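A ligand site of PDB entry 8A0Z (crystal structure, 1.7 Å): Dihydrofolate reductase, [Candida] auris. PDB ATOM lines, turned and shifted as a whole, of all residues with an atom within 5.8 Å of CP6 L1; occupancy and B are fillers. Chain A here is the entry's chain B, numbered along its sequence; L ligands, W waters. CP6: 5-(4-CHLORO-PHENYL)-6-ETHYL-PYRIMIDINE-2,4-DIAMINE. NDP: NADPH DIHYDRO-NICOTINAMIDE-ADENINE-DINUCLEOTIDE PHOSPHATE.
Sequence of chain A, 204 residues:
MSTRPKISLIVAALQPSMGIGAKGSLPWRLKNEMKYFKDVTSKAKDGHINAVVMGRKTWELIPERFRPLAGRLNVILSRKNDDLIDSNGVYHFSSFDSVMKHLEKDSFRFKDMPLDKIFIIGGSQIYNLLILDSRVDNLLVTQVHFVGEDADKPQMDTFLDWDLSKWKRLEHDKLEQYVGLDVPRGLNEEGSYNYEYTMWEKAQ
The side-chain hydroxyl (OH) of Tyr 127 lies within hydrogen-bond range of the backbone carbonyl oxygen (O) of Ile 121, at 3.1 Å.
N of Val 11 sits at hydrogen-bond distance from O of Leu 140 (3.0 Å).
OH of Tyr 127 sits at hydrogen-bond distance from O of Ile 10.
OE2 of Glu 33 sits at hydrogen-bond distance from OG1 of Thr 142 (2.6 Å).
The backbone NH (N) of Ile 10 sits at hydrogen-bond distance from the backbone carbonyl oxygen (O) of Ile 120 (3.1 Å).
N of Thr 142 sits at hydrogen-bond distance from O of Val 11 (2.8 Å).
Water W1 lies within hydrogen-bond range of the side-chain hydroxyl of Thr 142 (2.7 Å), the backbone carbonyl oxygen of Leu 140 (2.9 Å), a nitrogen (N14) of CP6 L1 (3.2 Å) and the backbone carbonyl oxygen of Val 11 (3.3 Å).
Residues that only touch CP6 L1: Val 11 (3.6 Å), Ala 12 (3.9 Å), Met 34 (3.8 Å), Phe 37 (3.5 Å), Thr 58 (3.6 Å) and Thr 142 (3.6 Å).
Hydrophobic or aromatic side chains within 4 Å of CP6 L1: Ile 10, Met 34, Phe 37 and Ile 121.
Within 4 Å of CP6 L1: Ile 10, Val 11, Ala 12, Glu 33, Met 34, Phe 37, Thr 58, Ile 121, Tyr 127 and Thr 142.
Along chain A the residues within 4 Å of CP6 L1 span positions 10 to 142.
The nearest printed residue that does not touch CP6 L1 is Leu 61 (4.03 Å).
N13 of CP6 L1 is in hydrogen-bond range of O of Ile 10 (2.9 Å).
The backbone carbonyl oxygen of Ala 12 lies within hydrogen-bond range of a nitrogen (N7N) of NDP L2.
The backbone NH (N) of Leu 26 sits at hydrogen-bond distance from an oxygen (O2D) of NDP L2 (3.4 Å).
The side-chain hydroxyl (OH) of Tyr 127 is in hydrogen-bond range of a nitrogen (N13) of CP6 L1, at 3.1 Å.
The side-chain hydroxyl (OH) of Tyr 127 lies close to an oxygen (O7N) of NDP L2, at 3.4 Å.
The side-chain carboxylate (OE2) of Glu 33 sits at hydrogen-bond distance from a nitrogen (N14) of CP6 L1 (2.7 Å).
The backbone NH (N) of Ala 12 sits at hydrogen-bond distance from an oxygen (O7N) of NDP L2, 2.9 Å away.
The side-chain hydroxyl of Thr 58 lies within hydrogen-bond range of an oxygen (O1A) of NDP L2 (2.7 Å).
A nitrogen (N13) of CP6 L1 is in hydrogen-bond range of the backbone carbonyl oxygen (O) of Ile 121 (2.9 Å).
The backbone NH (N) of Thr 58 lies within hydrogen-bond range of an oxygen (O1A) of NDP L2 (2.9 Å).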
ATOM      1  N   ILE A  10      26.103 -16.760 -27.991  1.00  0.00           N
ATOM      2  CA  ILE A  10      24.744 -17.048 -28.439  1.00  0.00           C
ATOM      3  C   ILE A  10      23.901 -15.789 -28.298  1.00  0.00           C
ATOM      4  O   ILE A  10      23.829 -15.208 -27.211  1.00  0.00           O
ATOM      5  CB  ILE A  10      24.122 -18.233 -27.686  1.00  0.00           C
ATOM      6  CG1 ILE A  10      22.756 -18.634 -28.286  1.00  0.00           C
ATOM      7  CG2 ILE A  10      24.031 -17.957 -26.156  1.00  0.00           C
ATOM      8  CD1 ILE A  10      22.261 -19.997 -27.757  1.00  0.00           C
ATOM      9  N   VAL A  11      23.258 -15.393 -29.392  1.00  0.00           N
ATOM     10  CA  VAL A  11      22.585 -14.091 -29.478  1.00  0.00           C
ATOM     11  C   VAL A  11      21.460 -14.175 -30.500  1.00  0.00           C
ATOM     12  O   VAL A  11      21.507 -14.973 -31.429  1.00  0.00           O
ATOM     13  CB  VAL A  11      23.610 -13.003 -29.862  1.00  0.00           C
ATOM     14  CG1 VAL A  11      24.238 -13.323 -31.238  1.00  0.00           C
ATOM     15  CG2 VAL A  11      22.957 -11.606 -29.829  1.00  0.00           C
ATOM     16  N   ALA A  12      20.435 -13.330 -30.303  1.00  0.00           N
ATOM     17  CA  ALA A  12      19.391 -13.134 -31.301  1.00  0.00           C
ATOM     18  C   ALA A  12      19.500 -11.697 -31.795  1.00  0.00           C
ATOM     19  O   ALA A  12      19.384 -10.756 -31.000  1.00  0.00           O
ATOM     20  CB  ALA A  12      18.009 -13.414 -30.710  1.00  0.00           C
ATOM     21  N   LEU A  26      14.520  -6.372 -24.718  1.00  0.00           N
ATOM     22  CA  LEU A  26      14.410  -7.100 -25.974  1.00  0.00           C
ATOM     23  C   LEU A  26      13.055  -6.828 -26.620  1.00  0.00           C
ATOM     24  O   LEU A  26      12.020  -7.122 -26.008  1.00  0.00           O
ATOM     25  CB  LEU A  26      14.592  -8.592 -25.713  1.00  0.00           C
ATOM     26  CG  LEU A  26      14.791  -9.493 -26.923  1.00  0.00           C
ATOM     27  CD1 LEU A  26      16.205  -9.317 -27.424  1.00  0.00           C
ATOM     28  CD2 LEU A  26      14.555 -10.950 -26.508  1.00  0.00           C
ATOM     29  N   GLU A  33      12.041 -19.334 -30.121  1.00  0.00           N
ATOM     30  CA  GLU A  33      13.427 -18.904 -29.997  1.00  0.00           C
ATOM     31  C   GLU A  33      13.885 -19.078 -28.554  1.00  0.00           C
ATOM     32  O   GLU A  33      14.974 -19.603 -28.289  1.00  0.00           O
ATOM     33  CB  GLU A  33      13.574 -17.450 -30.448  1.00  0.00           C
ATOM     34  CG  GLU A  33      14.899 -17.176 -31.112  1.00  0.00           C
ATOM     35  CD  GLU A  33      16.047 -16.993 -30.147  1.00  0.00           C
ATOM     36  OE1 GLU A  33      15.825 -16.438 -29.044  1.00  0.00           O
ATOM     37  OE2 GLU A  33      17.153 -17.477 -30.505  1.00  0.00           O
ATOM     38  N   MET A  34      13.022 -18.662 -27.615  1.00  0.00           N
ATOM     39  CA  MET A  34      13.197 -18.983 -26.205  1.00  0.00           C
ATOM     40  C   MET A  34      13.422 -20.466 -25.962  1.00  0.00           C
ATOM     41  O   MET A  34      14.324 -20.849 -25.198  1.00  0.00           O
ATOM     42  CB  MET A  34      11.971 -18.483 -25.428  1.00  0.00           C
ATOM     43  CG  MET A  34      12.110 -18.696 -23.948  1.00  0.00           C
ATOM     44  SD  MET A  34      13.534 -18.049 -23.097  1.00  0.00           S
ATOM     45  CE  MET A  34      13.734 -19.540 -22.136  1.00  0.00           C
ATOM     46  N   TYR A  36      14.543 -22.734 -28.020  1.00  0.00           N
ATOM     47  CA  TYR A  36      15.858 -23.043 -28.564  1.00  0.00           C
ATOM     48  C   TYR A  36      16.966 -22.622 -27.602  1.00  0.00           C
ATOM     49  O   TYR A  36      17.860 -23.410 -27.300  1.00  0.00           O
ATOM     50  CB  TYR A  36      16.029 -22.327 -29.906  1.00  0.00           C
ATOM     51  CG  TYR A  36      17.394 -22.391 -30.549  1.00  0.00           C
ATOM     52  CD1 TYR A  36      17.763 -23.498 -31.289  1.00  0.00           C
ATOM     53  CD2 TYR A  36      18.284 -21.332 -30.454  1.00  0.00           C
ATOM     54  CE1 TYR A  36      18.981 -23.553 -31.917  1.00  0.00           C
ATOM     55  CE2 TYR A  36      19.514 -21.379 -31.073  1.00  0.00           C
ATOM     56  CZ  TYR A  36      19.848 -22.492 -31.817  1.00  0.00           C
ATOM     57  OH  TYR A  36      21.082 -22.570 -32.455  1.00  0.00           O
ATOM     58  N   PHE A  37      16.925 -21.372 -27.145  1.00  0.00           N
ATOM     59  CA  PHE A  37      17.906 -20.896 -26.172  1.00  0.00           C
ATOM     60  C   PHE A  37      17.973 -21.826 -24.955  1.00  0.00           C
ATOM     61  O   PHE A  37      19.058 -22.234 -24.541  1.00  0.00           O
ATOM     62  CB  PHE A  37      17.568 -19.468 -25.727  1.00  0.00           C
ATOM     63  CG  PHE A  37      18.469 -18.949 -24.666  1.00  0.00           C
ATOM     64  CD1 PHE A  37      19.718 -18.476 -24.997  1.00  0.00           C
ATOM     65  CD2 PHE A  37      18.080 -18.968 -23.332  1.00  0.00           C
ATOM     66  CE1 PHE A  37      20.604 -18.013 -23.992  1.00  0.00           C
ATOM     67  CE2 PHE A  37      18.940 -18.515 -22.328  1.00  0.00           C
ATOM     68  CZ  PHE A  37      20.202 -18.017 -22.666  1.00  0.00           C
ATOM     69  N   THR A  58      22.175  -7.933 -17.868  1.00  0.00           N
ATOM     70  CA  THR A  58      21.376  -9.051 -18.382  1.00  0.00           C
ATOM     71  C   THR A  58      20.873  -9.917 -17.233  1.00  0.00           C
ATOM     72  O   THR A  58      19.699 -10.315 -17.214  1.00  0.00           O
ATOM     73  CB  THR A  58      22.209  -9.874 -19.372  1.00  0.00           C
ATOM     74  OG1 THR A  58      22.472  -9.092 -20.539  1.00  0.00           O
ATOM     75  CG2 THR A  58      21.489 -11.162 -19.783  1.00  0.00           C
ATOM     76  N   LEU A  61      17.988  -8.264 -15.978  1.00  0.00           N
ATOM     77  CA  LEU A  61      16.805  -8.363 -16.840  1.00  0.00           C
ATOM     78  C   LEU A  61      16.057  -9.684 -16.654  1.00  0.00           C
ATOM     79  O   LEU A  61      14.854  -9.742 -16.894  1.00  0.00           O
ATOM     80  CB  LEU A  61      17.151  -8.227 -18.315  1.00  0.00           C
ATOM     81  CG  LEU A  61      17.045  -6.889 -19.025  1.00  0.00           C
ATOM     82  CD1 LEU A  61      17.814  -6.929 -20.357  1.00  0.00           C
ATOM     83  CD2 LEU A  61      15.559  -6.574 -19.221  1.00  0.00           C
ATOM     84  N   ILE A  62      16.763 -10.752 -16.285  1.00  0.00           N
ATOM     85  CA  ILE A  62      16.124 -12.057 -16.174  1.00  0.00           C
ATOM     86  C   ILE A  62      15.148 -12.023 -15.006  1.00  0.00           C
ATOM     87  O   ILE A  62      15.552 -11.714 -13.882  1.00  0.00           O
ATOM     88  CB  ILE A  62      17.166 -13.162 -15.982  1.00  0.00           C
ATOM     89  CG1 ILE A  62      18.176 -13.128 -17.139  1.00  0.00           C
ATOM     90  CG2 ILE A  62      16.480 -14.504 -15.843  1.00  0.00           C
ATOM     91  CD1 ILE A  62      19.145 -14.290 -17.101  1.00  0.00           C
ATOM     92  N   ILE A 120      28.147 -17.484 -23.889  1.00  0.00           N
ATOM     93  CA  ILE A 120      28.105 -16.071 -23.540  1.00  0.00           C
ATOM     94  C   ILE A 120      26.737 -15.577 -23.982  1.00  0.00           C
ATOM     95  O   ILE A 120      26.432 -15.577 -25.178  1.00  0.00           O
ATOM     96  CB  ILE A 120      29.246 -15.287 -24.197  1.00  0.00           C
ATOM     97  CG1 ILE A 120      30.614 -15.763 -23.664  1.00  0.00           C
ATOM     98  CG2 ILE A 120      29.073 -13.767 -23.902  1.00  0.00           C
ATOM     99  CD1 ILE A 120      31.746 -15.660 -24.663  1.00  0.00           C
ATOM    100  N   ILE A 121      25.859 -15.261 -23.017  1.00  0.00           N
ATOM    101  CA  ILE A 121      24.457 -15.057 -23.362  1.00  0.00           C
ATOM    102  C   ILE A 121      24.048 -13.620 -23.303  1.00  0.00           C
ATOM    103  O   ILE A 121      22.861 -13.314 -23.498  1.00  0.00           O
ATOM    104  CB  ILE A 121      23.525 -15.882 -22.467  1.00  0.00           C
ATOM    105  CG1 ILE A 121      23.443 -15.231 -21.094  1.00  0.00           C
ATOM    106  CG2 ILE A 121      23.930 -17.330 -22.457  1.00  0.00           C
ATOM    107  CD1 ILE A 121      22.386 -15.833 -20.201  1.00  0.00           C
ATOM    108  N   GLY A 122      24.944 -12.703 -23.020  1.00  0.00           N
ATOM    109  CA  GLY A 122      24.274 -11.464 -22.744  1.00  0.00           C
ATOM    110  C   GLY A 122      25.089 -10.394 -22.099  1.00  0.00           C
ATOM    111  O   GLY A 122      26.055 -10.648 -21.375  1.00  0.00           O
ATOM    112  N   TYR A 127      28.971  -8.940 -24.966  1.00  0.00           N
ATOM    113  CA  TYR A 127      29.099  -9.419 -26.344  1.00  0.00           C
ATOM    114  C   TYR A 127      30.229  -8.699 -27.076  1.00  0.00           C
ATOM    115  O   TYR A 127      31.043  -9.313 -27.760  1.00  0.00           O
ATOM    116  CB  TYR A 127      27.811  -9.173 -27.121  1.00  0.00           C
ATOM    117  CG  TYR A 127      26.648 -10.113 -26.929  1.00  0.00           C
ATOM    118  CD1 TYR A 127      26.818 -11.493 -26.703  1.00  0.00           C
ATOM    119  CD2 TYR A 127      25.349  -9.620 -26.999  1.00  0.00           C
ATOM    120  CE1 TYR A 127      25.711 -12.321 -26.545  1.00  0.00           C
ATOM    121  CE2 TYR A 127      24.266 -10.433 -26.832  1.00  0.00           C
ATOM    122  CZ  TYR A 127      24.440 -11.784 -26.617  1.00  0.00           C
ATOM    123  OH  TYR A 127      23.323 -12.567 -26.479  1.00  0.00           O
ATOM    124  N   LEU A 140      26.523 -18.567 -32.225  1.00  0.00           N
ATOM    125  CA  LEU A 140      25.185 -19.095 -32.476  1.00  0.00           C
ATOM    126  C   LEU A 140      24.284 -17.872 -32.581  1.00  0.00           C
ATOM    127  O   LEU A 140      23.860 -17.300 -31.563  1.00  0.00           O
ATOM    128  CB  LEU A 140      24.762 -20.047 -31.367  1.00  0.00           C
ATOM    129  CG  LEU A 140      25.476 -21.412 -31.380  1.00  0.00           C
ATOM    130  CD1 LEU A 140      25.235 -22.120 -30.053  1.00  0.00           C
ATOM    131  CD2 LEU A 140      25.030 -22.293 -32.547  1.00  0.00           C
ATOM    132  N   THR A 142      20.854 -16.256 -33.888  1.00  0.00           N
ATOM    133  CA  THR A 142      19.516 -16.321 -34.441  1.00  0.00           C
ATOM    134  C   THR A 142      19.293 -15.050 -35.254  1.00  0.00           C
ATOM    135  O   THR A 142      19.222 -13.942 -34.702  1.00  0.00           O
ATOM    136  CB  THR A 142      18.457 -16.480 -33.353  1.00  0.00           C
ATOM    137  OG1 THR A 142      18.733 -17.670 -32.607  1.00  0.00           O
ATOM    138  CG2 THR A 142      17.068 -16.586 -34.008  1.00  0.00           C
HETATM  139  N1  CP6 L   1      20.319 -15.879 -27.280  1.00  0.00           N
HETATM  140  C2  CP6 L   1      19.244 -16.263 -27.956  1.00  0.00           C
HETATM  141  C3  CP6 L   1      20.243 -15.173 -26.167  1.00  0.00           C
HETATM  142  C4  CP6 L   1      18.953 -14.846 -25.713  1.00  0.00           C
HETATM  143  C5  CP6 L   1      17.799 -15.204 -26.392  1.00  0.00           C
HETATM  144  N6  CP6 L   1      18.062 -15.904 -27.485  1.00  0.00           N
HETATM  145  C7  CP6 L   1      18.766 -13.999 -24.435  1.00  0.00           C
HETATM  146  C8  CP6 L   1      18.205 -12.732 -24.565  1.00  0.00           C
HETATM  147  C9  CP6 L   1      17.987 -11.893 -23.475  1.00  0.00           C
HETATM  148  C10 CP6 L   1      18.374 -12.323 -22.225  1.00  0.00           C
HETATM  149  C11 CP6 L   1      18.923 -13.600 -22.072  1.00  0.00           C
HETATM  150  C12 CP6 L   1      19.134 -14.439 -23.174  1.00  0.00           C
HETATM  151  N13 CP6 L   1      21.500 -14.826 -25.543  1.00  0.00           N
HETATM  152  N14 CP6 L   1      19.404 -17.025 -29.152  1.00  0.00           N
HETATM  153  C15 CP6 L   1      16.373 -14.895 -25.954  1.00  0.00           C
HETATM  154  C16 CP6 L   1      15.749 -16.215 -25.530  1.00  0.00           C
HETATM  155 CL1  CP6 L   1      18.092 -11.238 -20.818  1.00  0.00          CL
HETATM  156  PA  NDP L   2      25.301  -6.231 -19.983  1.00  0.00           P
HETATM  157  O1A NDP L   2      24.320  -7.326 -19.774  1.00  0.00           O
HETATM  158  O2A NDP L   2      26.427  -6.367 -20.976  1.00  0.00           O
HETATM  159  O5B NDP L   2      25.934  -5.998 -18.517  1.00  0.00           O
HETATM  160  C5B NDP L   2      26.571  -4.749 -18.552  1.00  0.00           C
HETATM  161  C4B NDP L   2      27.364  -4.743 -17.263  1.00  0.00           C
HETATM  162  O4B NDP L   2      28.389  -5.668 -17.418  1.00  0.00           O
HETATM  163  C3B NDP L   2      28.034  -3.381 -16.956  1.00  0.00           C
HETATM  164  O3B NDP L   2      27.149  -2.504 -16.322  1.00  0.00           O
HETATM  165  C2B NDP L   2      29.067  -3.857 -15.947  1.00  0.00           C
HETATM  166  O2B NDP L   2      28.585  -4.101 -14.736  1.00  0.00           O
HETATM  167  C1B NDP L   2      29.454  -5.229 -16.580  1.00  0.00           C
HETATM  168  N9A NDP L   2      30.655  -5.079 -17.357  1.00  0.00           N
HETATM  169  C8A NDP L   2      30.867  -4.225 -18.486  1.00  0.00           C
HETATM  170  N7A NDP L   2      32.131  -4.311 -18.952  1.00  0.00           N
HETATM  171  C5A NDP L   2      32.759  -5.241 -18.073  1.00  0.00           C
HETATM  172  C6A NDP L   2      34.057  -5.750 -18.018  1.00  0.00           C
HETATM  173  N6A NDP L   2      34.990  -5.333 -18.959  1.00  0.00           N
HETATM  174  N1A NDP L   2      34.438  -6.674 -17.065  1.00  0.00           N
HETATM  175  C2A NDP L   2      33.454  -7.036 -16.178  1.00  0.00           C
HETATM  176  N3A NDP L   2      32.168  -6.641 -16.098  1.00  0.00           N
HETATM  177  C4A NDP L   2      31.842  -5.720 -17.084  1.00  0.00           C
HETATM  178  O3  NDP L   2      24.322  -4.901 -20.165  1.00  0.00           O
HETATM  179  PN  NDP L   2      24.098  -4.201 -21.591  1.00  0.00           P
HETATM  180  O1N NDP L   2      23.121  -3.130 -21.301  1.00  0.00           O
HETATM  181  O2N NDP L   2      25.300  -3.933 -22.469  1.00  0.00           O
HETATM  182  O5D NDP L   2      23.197  -5.271 -22.522  1.00  0.00           O
HETATM  183  C5D NDP L   2      21.882  -5.089 -22.200  1.00  0.00           C
HETATM  184  C4D NDP L   2      21.136  -5.021 -23.510  1.00  0.00           C
HETATM  185  O4D NDP L   2      21.442  -6.199 -24.244  1.00  0.00           O
HETATM  186  C3D NDP L   2      19.596  -5.013 -23.289  1.00  0.00           C
HETATM  187  O3D NDP L   2      19.046  -4.200 -24.271  1.00  0.00           O
HETATM  188  C2D NDP L   2      19.217  -6.442 -23.574  1.00  0.00           C
HETATM  189  O2D NDP L   2      17.904  -6.515 -24.110  1.00  0.00           O
HETATM  190  C1D NDP L   2      20.226  -6.774 -24.717  1.00  0.00           C
HETATM  191  N1N NDP L   2      20.399  -8.244 -24.815  1.00  0.00           N
HETATM  192  C2N NDP L   2      20.097  -8.891 -26.005  1.00  0.00           C
HETATM  193  C3N NDP L   2      20.390 -10.219 -26.160  1.00  0.00           C
HETATM  194  C7N NDP L   2      20.012 -10.844 -27.437  1.00  0.00           C
HETATM  195  O7N NDP L   2      20.262 -12.034 -27.741  1.00  0.00           O
HETATM  196  N7N NDP L   2      19.301 -10.068 -28.346  1.00  0.00           N
HETATM  197  C4N NDP L   2      21.064 -11.046 -25.063  1.00  0.00           C
HETATM  198  C5N NDP L   2      21.233 -10.294 -23.785  1.00  0.00           C
HETATM  199  C6N NDP L   2      20.918  -8.987 -23.691  1.00  0.00           C
HETATM  200  P2B NDP L   2      29.409  -3.220 -13.417  1.00  0.00           P
HETATM  201  O1X NDP L   2      30.813  -3.635 -13.675  1.00  0.00           O
HETATM  202  O2X NDP L   2      28.722  -3.777 -12.162  1.00  0.00           O
HETATM  203  O3X NDP L   2      29.033  -1.810 -13.800  1.00  0.00           O
HETATM  204  O   HOH W   1      21.142 -18.237 -31.488  1.00  0.00           O
